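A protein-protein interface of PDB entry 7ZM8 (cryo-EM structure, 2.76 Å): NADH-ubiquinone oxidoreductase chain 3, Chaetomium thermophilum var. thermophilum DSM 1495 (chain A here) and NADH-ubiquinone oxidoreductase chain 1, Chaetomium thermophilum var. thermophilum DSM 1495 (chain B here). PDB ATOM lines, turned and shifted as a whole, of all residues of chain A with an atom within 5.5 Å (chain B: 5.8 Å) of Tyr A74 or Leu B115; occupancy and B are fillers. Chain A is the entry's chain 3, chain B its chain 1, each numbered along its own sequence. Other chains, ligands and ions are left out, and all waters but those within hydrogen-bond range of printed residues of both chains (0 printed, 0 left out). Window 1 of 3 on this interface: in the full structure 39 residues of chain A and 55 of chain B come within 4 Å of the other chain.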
ATOM      1  N   ILE A  70     -30.536 -16.306 -23.991  1.00  0.00           N
ATOM      2  CA  ILE A  70     -29.553 -16.503 -22.931  1.00  0.00           C
ATOM      3  C   ILE A  70     -29.004 -15.163 -22.465  1.00  0.00           C
ATOM      4  O   ILE A  70     -28.725 -14.969 -21.278  1.00  0.00           O
ATOM      5  CB  ILE A  70     -28.435 -17.457 -23.405  1.00  0.00           C
ATOM      6  CG1 ILE A  70     -28.889 -18.911 -23.288  1.00  0.00           C
ATOM      7  CG2 ILE A  70     -27.147 -17.260 -22.617  1.00  0.00           C
ATOM      8  CD1 ILE A  70     -29.155 -19.345 -21.872  1.00  0.00           C
ATOM      9  N   LEU A  71     -28.853 -14.214 -23.391  1.00  0.00           N
ATOM     10  CA  LEU A  71     -28.413 -12.874 -23.022  1.00  0.00           C
ATOM     11  C   LEU A  71     -29.396 -12.212 -22.068  1.00  0.00           C
ATOM     12  O   LEU A  71     -28.989 -11.563 -21.100  1.00  0.00           O
ATOM     13  CB  LEU A  71     -28.241 -12.015 -24.272  1.00  0.00           C
ATOM     14  CG  LEU A  71     -27.717 -10.595 -24.027  1.00  0.00           C
ATOM     15  CD1 LEU A  71     -26.320 -10.614 -23.425  1.00  0.00           C
ATOM     16  CD2 LEU A  71     -27.773  -9.749 -25.286  1.00  0.00           C
ATOM     17  N   LEU A  72     -30.695 -12.357 -22.329  1.00  0.00           N
ATOM     18  CA  LEU A  72     -31.709 -11.728 -21.493  1.00  0.00           C
ATOM     19  C   LEU A  72     -31.753 -12.323 -20.094  1.00  0.00           C
ATOM     20  O   LEU A  72     -32.342 -11.718 -19.196  1.00  0.00           O
ATOM     21  CB  LEU A  72     -33.081 -11.850 -22.154  1.00  0.00           C
ATOM     22  CG  LEU A  72     -33.326 -11.034 -23.425  1.00  0.00           C
ATOM     23  CD1 LEU A  72     -34.215 -11.807 -24.371  1.00  0.00           C
ATOM     24  CD2 LEU A  72     -33.932  -9.678 -23.127  1.00  0.00           C
ATOM     25  N   LEU A  73     -31.141 -13.486 -19.889  1.00  0.00           N
ATOM     26  CA  LEU A  73     -31.069 -14.115 -18.579  1.00  0.00           C
ATOM     27  C   LEU A  73     -29.858 -13.679 -17.766  1.00  0.00           C
ATOM     28  O   LEU A  73     -29.869 -13.825 -16.542  1.00  0.00           O
ATOM     29  CB  LEU A  73     -31.048 -15.635 -18.735  1.00  0.00           C
ATOM     30  CG  LEU A  73     -32.390 -16.315 -18.961  1.00  0.00           C
ATOM     31  CD1 LEU A  73     -32.171 -17.788 -19.184  1.00  0.00           C
ATOM     32  CD2 LEU A  73     -33.306 -16.072 -17.773  1.00  0.00           C
ATOM     33  N   TYR A  74     -28.821 -13.157 -18.415  1.00  0.00           N
ATOM     34  CA  TYR A  74     -27.643 -12.702 -17.683  1.00  0.00           C
ATOM     35  C   TYR A  74     -27.936 -11.612 -16.658  1.00  0.00           C
ATOM     36  O   TYR A  74     -27.300 -11.635 -15.590  1.00  0.00           O
ATOM     37  CB  TYR A  74     -26.561 -12.247 -18.669  1.00  0.00           C
ATOM     38  CG  TYR A  74     -25.598 -13.349 -19.032  1.00  0.00           C
ATOM     39  CD1 TYR A  74     -25.881 -14.227 -20.063  1.00  0.00           C
ATOM     40  CD2 TYR A  74     -24.421 -13.531 -18.324  1.00  0.00           C
ATOM     41  CE1 TYR A  74     -25.018 -15.240 -20.392  1.00  0.00           C
ATOM     42  CE2 TYR A  74     -23.548 -14.549 -18.646  1.00  0.00           C
ATOM     43  CZ  TYR A  74     -23.855 -15.401 -19.684  1.00  0.00           C
ATOM     44  OH  TYR A  74     -22.998 -16.417 -20.023  1.00  0.00           O
ATOM     45  N   PRO A  75     -28.809 -10.630 -16.909  1.00  0.00           N
ATOM     46  CA  PRO A  75     -29.141  -9.684 -15.835  1.00  0.00           C
ATOM     47  C   PRO A  75     -29.752 -10.336 -14.611  1.00  0.00           C
ATOM     48  O   PRO A  75     -29.552  -9.839 -13.499  1.00  0.00           O
ATOM     49  CB  PRO A  75     -30.121  -8.722 -16.517  1.00  0.00           C
ATOM     50  CG  PRO A  75     -29.798  -8.811 -17.936  1.00  0.00           C
ATOM     51  CD  PRO A  75     -29.432 -10.225 -18.181  1.00  0.00           C
ATOM     52  N   PHE A  76     -30.494 -11.431 -14.777  1.00  0.00           N
ATOM     53  CA  PHE A  76     -31.087 -12.101 -13.627  1.00  0.00           C
ATOM     54  C   PHE A  76     -30.021 -12.678 -12.712  1.00  0.00           C
ATOM     55  O   PHE A  76     -30.156 -12.629 -11.486  1.00  0.00           O
ATOM     56  CB  PHE A  76     -32.039 -13.203 -14.090  1.00  0.00           C
ATOM     57  CG  PHE A  76     -32.641 -13.986 -12.966  1.00  0.00           C
ATOM     58  CD1 PHE A  76     -33.723 -13.495 -12.272  1.00  0.00           C
ATOM     59  CD2 PHE A  76     -32.110 -15.208 -12.596  1.00  0.00           C
ATOM     60  CE1 PHE A  76     -34.264 -14.206 -11.233  1.00  0.00           C
ATOM     61  CE2 PHE A  76     -32.651 -15.921 -11.557  1.00  0.00           C
ATOM     62  CZ  PHE A  76     -33.731 -15.421 -10.877  1.00  0.00           C
ATOM     63  N   ALA A  77     -28.958 -13.239 -13.289  1.00  0.00           N
ATOM     64  CA  ALA A  77     -27.923 -13.884 -12.495  1.00  0.00           C
ATOM     65  C   ALA A  77     -27.150 -12.902 -11.628  1.00  0.00           C
ATOM     66  O   ALA A  77     -26.694 -13.280 -10.547  1.00  0.00           O
ATOM     67  CB  ALA A  77     -26.963 -14.641 -13.404  1.00  0.00           C
ATOM     68  N   VAL A  78     -26.993 -11.655 -12.068  1.00  0.00           N
ATOM     69  CA  VAL A  78     -26.307 -10.644 -11.279  1.00  0.00           C
ATOM     70  C   VAL A  78     -27.286  -9.747 -10.534  1.00  0.00           C
ATOM     71  O   VAL A  78     -26.912  -8.662 -10.090  1.00  0.00           O
ATOM     72  CB  VAL A  78     -25.345  -9.813 -12.147  1.00  0.00           C
ATOM     73  CG1 VAL A  78     -24.214 -10.673 -12.647  1.00  0.00           C
ATOM     74  CG2 VAL A  78     -26.076  -9.194 -13.318  1.00  0.00           C
ATOM     75  N   GLY B 110     -16.446  -8.489 -16.595  1.00  0.00           N
ATOM     76  CA  GLY B 110     -15.352  -9.220 -17.210  1.00  0.00           C
ATOM     77  C   GLY B 110     -15.807 -10.414 -18.022  1.00  0.00           C
ATOM     78  O   GLY B 110     -15.186 -10.750 -19.032  1.00  0.00           O
ATOM     79  N   ILE B 111     -16.876 -11.079 -17.588  1.00  0.00           N
ATOM     80  CA  ILE B 111     -17.389 -12.240 -18.306  1.00  0.00           C
ATOM     81  C   ILE B 111     -17.995 -11.828 -19.643  1.00  0.00           C
ATOM     82  O   ILE B 111     -17.721 -12.441 -20.680  1.00  0.00           O
ATOM     83  CB  ILE B 111     -18.404 -12.994 -17.430  1.00  0.00           C
ATOM     84  CG1 ILE B 111     -17.684 -13.752 -16.324  1.00  0.00           C
ATOM     85  CG2 ILE B 111     -19.220 -13.950 -18.266  1.00  0.00           C
ATOM     86  CD1 ILE B 111     -16.855 -14.904 -16.822  1.00  0.00           C
ATOM     87  N   LEU B 112     -18.839 -10.794 -19.641  1.00  0.00           N
ATOM     88  CA  LEU B 112     -19.394 -10.300 -20.895  1.00  0.00           C
ATOM     89  C   LEU B 112     -18.328  -9.721 -21.811  1.00  0.00           C
ATOM     90  O   LEU B 112     -18.539  -9.661 -23.025  1.00  0.00           O
ATOM     91  CB  LEU B 112     -20.488  -9.262 -20.637  1.00  0.00           C
ATOM     92  CG  LEU B 112     -21.917  -9.724 -20.338  1.00  0.00           C
ATOM     93  CD1 LEU B 112     -22.479 -10.444 -21.541  1.00  0.00           C
ATOM     94  CD2 LEU B 112     -22.007 -10.621 -19.131  1.00  0.00           C
ATOM     95  N   TYR B 113     -17.162  -9.365 -21.269  1.00  0.00           N
ATOM     96  CA  TYR B 113     -16.045  -8.913 -22.140  1.00  0.00           C
ATOM     97  C   TYR B 113     -15.526 -10.117 -22.920  1.00  0.00           C
ATOM     98  O   TYR B 113     -15.264  -9.992 -24.124  1.00  0.00           O
ATOM     99  CB  TYR B 113     -14.918  -8.286 -21.316  1.00  0.00           C
ATOM    100  CG  TYR B 113     -13.699  -7.948 -22.133  1.00  0.00           C
ATOM    101  CD1 TYR B 113     -13.677  -6.831 -22.950  1.00  0.00           C
ATOM    102  CD2 TYR B 113     -12.580  -8.762 -22.121  1.00  0.00           C
ATOM    103  CE1 TYR B 113     -12.568  -6.523 -23.719  1.00  0.00           C
ATOM    104  CE2 TYR B 113     -11.462  -8.468 -22.880  1.00  0.00           C
ATOM    105  CZ  TYR B 113     -11.457  -7.344 -23.684  1.00  0.00           C
ATOM    106  OH  TYR B 113     -10.361  -7.047 -24.439  1.00  0.00           O
ATOM    107  N   MET B 114     -15.355 -11.244 -22.231  1.00  0.00           N
ATOM    108  CA  MET B 114     -14.828 -12.480 -22.869  1.00  0.00           C
ATOM    109  C   MET B 114     -15.807 -13.055 -23.902  1.00  0.00           C
ATOM    110  O   MET B 114     -15.344 -13.586 -24.923  1.00  0.00           O
ATOM    111  CB  MET B 114     -14.421 -13.521 -21.828  1.00  0.00           C
ATOM    112  CG  MET B 114     -12.989 -13.328 -21.373  1.00  0.00           C
ATOM    113  SD  MET B 114     -12.605 -14.299 -19.908  1.00  0.00           S
ATOM    114  CE  MET B 114     -14.102 -14.024 -18.967  1.00  0.00           C
ATOM    115  N   LEU B 115     -17.108 -12.979 -23.637  1.00  0.00           N
ATOM    116  CA  LEU B 115     -18.121 -13.453 -24.614  1.00  0.00           C
ATOM    117  C   LEU B 115     -18.024 -12.622 -25.898  1.00  0.00           C
ATOM    118  O   LEU B 115     -18.166 -13.208 -26.985  1.00  0.00           O
ATOM    119  CB  LEU B 115     -19.507 -13.353 -23.972  1.00  0.00           C
ATOM    120  CG  LEU B 115     -19.771 -14.321 -22.821  1.00  0.00           C
ATOM    121  CD1 LEU B 115     -21.173 -14.130 -22.267  1.00  0.00           C
ATOM    122  CD2 LEU B 115     -19.568 -15.759 -23.269  1.00  0.00           C
ATOM    123  N   ALA B 116     -17.804 -11.310 -25.772  1.00  0.00           N
ATOM    124  CA  ALA B 116     -17.676 -10.425 -26.954  1.00  0.00           C
ATOM    125  C   ALA B 116     -16.451 -10.794 -27.799  1.00  0.00           C
ATOM    126  O   ALA B 116     -16.575 -10.822 -29.037  1.00  0.00           O
ATOM    127  CB  ALA B 116     -17.637  -8.981 -26.526  1.00  0.00           C
ATOM    128  N   VAL B 117     -15.331 -11.118 -27.145  1.00  0.00           N
ATOM    129  CA  VAL B 117     -14.076 -11.458 -27.881  1.00  0.00           C
ATOM    130  C   VAL B 117     -14.227 -12.815 -28.573  1.00  0.00           C
ATOM    131  O   VAL B 117     -13.610 -12.996 -29.634  1.00  0.00           O
ATOM    132  CB  VAL B 117     -12.790 -11.322 -27.037  1.00  0.00           C
ATOM    133  CG1 VAL B 117     -12.629  -9.926 -26.455  1.00  0.00           C
ATOM    134  CG2 VAL B 117     -12.656 -12.381 -25.956  1.00  0.00           C
ATOM    135  N   SER B 118     -15.009 -13.728 -27.990  1.00  0.00           N
ATOM    136  CA  SER B 118     -15.261 -15.061 -28.597  1.00  0.00           C
ATOM    137  C   SER B 118     -16.106 -14.917 -29.862  1.00  0.00           C
ATOM    138  O   SER B 118     -15.809 -15.602 -30.859  1.00  0.00           O
ATOM    139  CB  SER B 118     -15.941 -15.959 -27.616  1.00  0.00           C
ATOM    140  OG  SER B 118     -15.873 -17.308 -28.047  1.00  0.00           O
ATOM    141  N   SER B 119     -17.125 -14.059 -29.814  1.00  0.00           N
ATOM    142  CA  SER B 119     -18.019 -13.855 -30.979  1.00  0.00           C
ATOM    143  C   SER B 119     -17.203 -13.270 -32.136  1.00  0.00           C
ATOM    144  O   SER B 119     -17.465 -13.650 -33.291  1.00  0.00           O
ATOM    145  CB  SER B 119     -19.193 -12.997 -30.599  1.00  0.00           C
ATOM    146  OG  SER B 119     -18.775 -11.708 -30.182  1.00  0.00           O
ATOM    147  N   LEU B 120     -16.265 -12.369 -31.836  1.00  0.00           N
ATOM    148  CA  LEU B 120     -15.383 -11.771 -32.875  1.00  0.00           C
ATOM    149  C   LEU B 120     -14.502 -12.852 -33.504  1.00  0.00           C
ATOM    150  O   LEU B 120     -14.206 -12.735 -34.704  1.00  0.00           O
ATOM    151  CB  LEU B 120     -14.533 -10.674 -32.229  1.00  0.00           C
ATOM    152  CG  LEU B 120     -15.261  -9.367 -31.928  1.00  0.00           C
ATOM    153  CD1 LEU B 120     -14.455  -8.509 -30.966  1.00  0.00           C
ATOM    154  CD2 LEU B 120     -15.547  -8.607 -33.212  1.00  0.00           C
ATOM    155  N   GLU B 152     -20.557 -22.044 -28.792  1.00  0.00           N
ATOM    156  CA  GLU B 152     -20.481 -20.772 -28.024  1.00  0.00           C
ATOM    157  C   GLU B 152     -21.713 -20.694 -27.127  1.00  0.00           C
ATOM    158  O   GLU B 152     -21.586 -20.224 -25.991  1.00  0.00           O
ATOM    159  CB  GLU B 152     -20.361 -19.574 -28.964  1.00  0.00           C
ATOM    160  CG  GLU B 152     -20.227 -18.242 -28.248  1.00  0.00           C
ATOM    161  CD  GLU B 152     -19.020 -18.093 -27.335  1.00  0.00           C
ATOM    162  OE1 GLU B 152     -19.024 -17.159 -26.509  1.00  0.00           O
ATOM    163  OE2 GLU B 152     -18.073 -18.896 -27.458  1.00  0.00           O
ATOM    164  N   LEU B 155     -21.051 -22.762 -24.228  1.00  0.00           N
ATOM    165  CA  LEU B 155     -20.103 -22.061 -23.320  1.00  0.00           C
ATOM    166  C   LEU B 155     -20.802 -20.925 -22.578  1.00  0.00           C
ATOM    167  O   LEU B 155     -20.518 -20.749 -21.387  1.00  0.00           O
ATOM    168  CB  LEU B 155     -18.903 -21.546 -24.119  1.00  0.00           C
ATOM    169  CG  LEU B 155     -17.953 -22.624 -24.636  1.00  0.00           C
ATOM    170  CD1 LEU B 155     -16.686 -22.003 -25.199  1.00  0.00           C
ATOM    171  CD2 LEU B 155     -17.614 -23.616 -23.538  1.00  0.00           C
ATOM    172  N   SER B 156     -21.718 -20.220 -23.239  1.00  0.00           N
ATOM    173  CA  SER B 156     -22.334 -19.019 -22.620  1.00  0.00           C
ATOM    174  C   SER B 156     -23.461 -19.455 -21.687  1.00  0.00           C
ATOM    175  O   SER B 156     -23.635 -18.819 -20.641  1.00  0.00           O
ATOM    176  CB  SER B 156     -22.845 -18.088 -23.684  1.00  0.00           C
ATOM    177  OG  SER B 156     -23.892 -18.691 -24.426  1.00  0.00           O
ATOM    178  N   SER B 157     -24.176 -20.521 -22.037  1.00  0.00           N
ATOM    179  CA  SER B 157     -25.215 -21.035 -21.153  1.00  0.00           C
ATOM    180  C   SER B 157     -24.622 -21.649 -19.893  1.00  0.00           C
ATOM    181  O   SER B 157     -25.206 -21.541 -18.810  1.00  0.00           O
ATOM    182  CB  SER B 157     -26.068 -22.066 -21.888  1.00  0.00           C
ATOM    183  OG  SER B 157     -26.581 -21.534 -23.088  1.00  0.00           O
ATOM    184  N   ILE B 159     -21.587 -20.743 -18.508  1.00  0.00           N
ATOM    185  CA  ILE B 159     -21.012 -19.639 -17.682  1.00  0.00           C
ATOM    186  C   ILE B 159     -22.147 -19.050 -16.847  1.00  0.00           C
ATOM    187  O   ILE B 159     -21.902 -18.707 -15.679  1.00  0.00           O
ATOM    188  CB  ILE B 159     -20.319 -18.583 -18.568  1.00  0.00           C
ATOM    189  CG1 ILE B 159     -18.991 -19.094 -19.127  1.00  0.00           C
ATOM    190  CG2 ILE B 159     -20.127 -17.283 -17.812  1.00  0.00           C
ATOM    191  CD1 ILE B 159     -18.296 -18.119 -20.047  1.00  0.00           C
ATOM    192  N   LEU B 160     -23.353 -19.003 -17.413  1.00  0.00           N
ATOM    193  CA  LEU B 160     -24.515 -18.407 -16.712  1.00  0.00           C
ATOM    194  C   LEU B 160     -24.777 -19.198 -15.423  1.00  0.00           C
ATOM    195  O   LEU B 160     -25.323 -18.604 -14.481  1.00  0.00           O
ATOM    196  CB  LEU B 160     -25.724 -18.462 -17.654  1.00  0.00           C
ATOM    197  CG  LEU B 160     -27.016 -17.831 -17.139  1.00  0.00           C
ATOM    198  CD1 LEU B 160     -26.833 -16.343 -16.899  1.00  0.00           C
ATOM    199  CD2 LEU B 160     -28.153 -18.075 -18.116  1.00  0.00           C
ATOM    200  N   ILE B 163     -22.284 -17.766 -12.821  1.00  0.00           N
ATOM    201  CA  ILE B 163     -22.678 -16.421 -12.418  1.00  0.00           C
ATOM    202  C   ILE B 163     -23.803 -16.468 -11.400  1.00  0.00           C
ATOM    203  O   ILE B 163     -23.891 -15.604 -10.520  1.00  0.00           O
ATOM    204  CB  ILE B 163     -23.069 -15.598 -13.661  1.00  0.00           C
ATOM    205  CG1 ILE B 163     -21.979 -15.699 -14.736  1.00  0.00           C
ATOM    206  CG2 ILE B 163     -23.328 -14.147 -13.289  1.00  0.00           C
ATOM    207  CD1 ILE B 163     -20.639 -15.136 -14.326  1.00  0.00           C
ATOM    208  N   LEU B 169     -19.966 -10.857 -12.468  1.00  0.00           N
ATOM    209  CA  LEU B 169     -19.275 -11.167 -13.747  1.00  0.00           C
ATOM    210  C   LEU B 169     -17.809 -10.740 -13.642  1.00  0.00           C
ATOM    211  O   LEU B 169     -17.128 -10.849 -14.647  1.00  0.00           O
ATOM    212  CB  LEU B 169     -19.961 -10.396 -14.877  1.00  0.00           C
ATOM    213  CG  LEU B 169     -21.471 -10.559 -15.014  1.00  0.00           C
ATOM    214  CD1 LEU B 169     -22.070  -9.351 -15.708  1.00  0.00           C
ATOM    215  CD2 LEU B 169     -21.819 -11.830 -15.766  1.00  0.00           C
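The backbone carbonyl oxygen (O) of Ser B156 sits at hydrogen-bond distance from the side-chain hydroxyl (OH) of Tyr A74.
The backbone NH (N) of Ile B111 is in hydrogen-bond range of the backbone carbonyl oxygen (O) of Leu B169, 3.0 Å away.
The side-chain hydroxyl of Ser B156 sits at hydrogen-bond distance from the backbone carbonyl oxygen of Glu B152, 3.2 Å away.
The backbone NH (N) of Gly B110 lies within hydrogen-bond range of the backbone carbonyl oxygen (O) of Leu B169 (3.1 Å).
Among the printed residues, pairs that only touch across the chains: Ile A70 with Ser B156, Ile A70 with Ser B157, Leu A73 with Leu B160, Tyr A74 with Leu B112, Tyr A74 with Leu B115, Tyr A74 with Ile B159, Tyr A74 with Leu B160, Ala A77 with Leu B160, Ala A77 with Ile B163, Val A78 with Ile B163 and Val A78 with Leu B169.
Tyr A74 touches five residues of chain B.
Leu B115 touches just one residue of chain A: Tyr A74.
Printed residues of chain A within 4 Å of Leu B112: Tyr A74 (3.9 Å).
Of the printed residues of chain A, Ser B157 touches Ile A70.
Phe A76 touches none of the printed residues of chain B.
The nearest residue of chain B that does not touch Tyr A74 is Leu B169 (4.03 Å).
The nearest printed residue of chain A that does not touch Leu B115 is Leu A71 (6.3 Å).
The nearest printed residue of chain B that does not touch Val A78 is Leu B160 (6.7 Å).
Of the 9 printed residues of chain A, 5 touch a printed residue of chain B.
Printed residues of chain A that touch a printed residue of chain B: Ile A70, Leu A73, Tyr A74, Ala A77 and Val A78.
Hydrophobic or aromatic side chains of chain A within 4 Å of the printed part of chain B: Ile A70, Leu A73, Tyr A74, Ala A77 and Val A78.
Printed residues of chain B that touch a printed residue of chain A: Leu B112, Leu B115, Ser B156, Ser B157, Ile B159, Leu B160, Ile B163 and Leu B169.
Along chain B the printed residues that touch a printed residue of chain A span positions 112 to 169.
Among the printed residues, no Asp or Glu carboxylate lies within 4 Å of a Lys or Arg side-chain nitrogen of the other chain.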
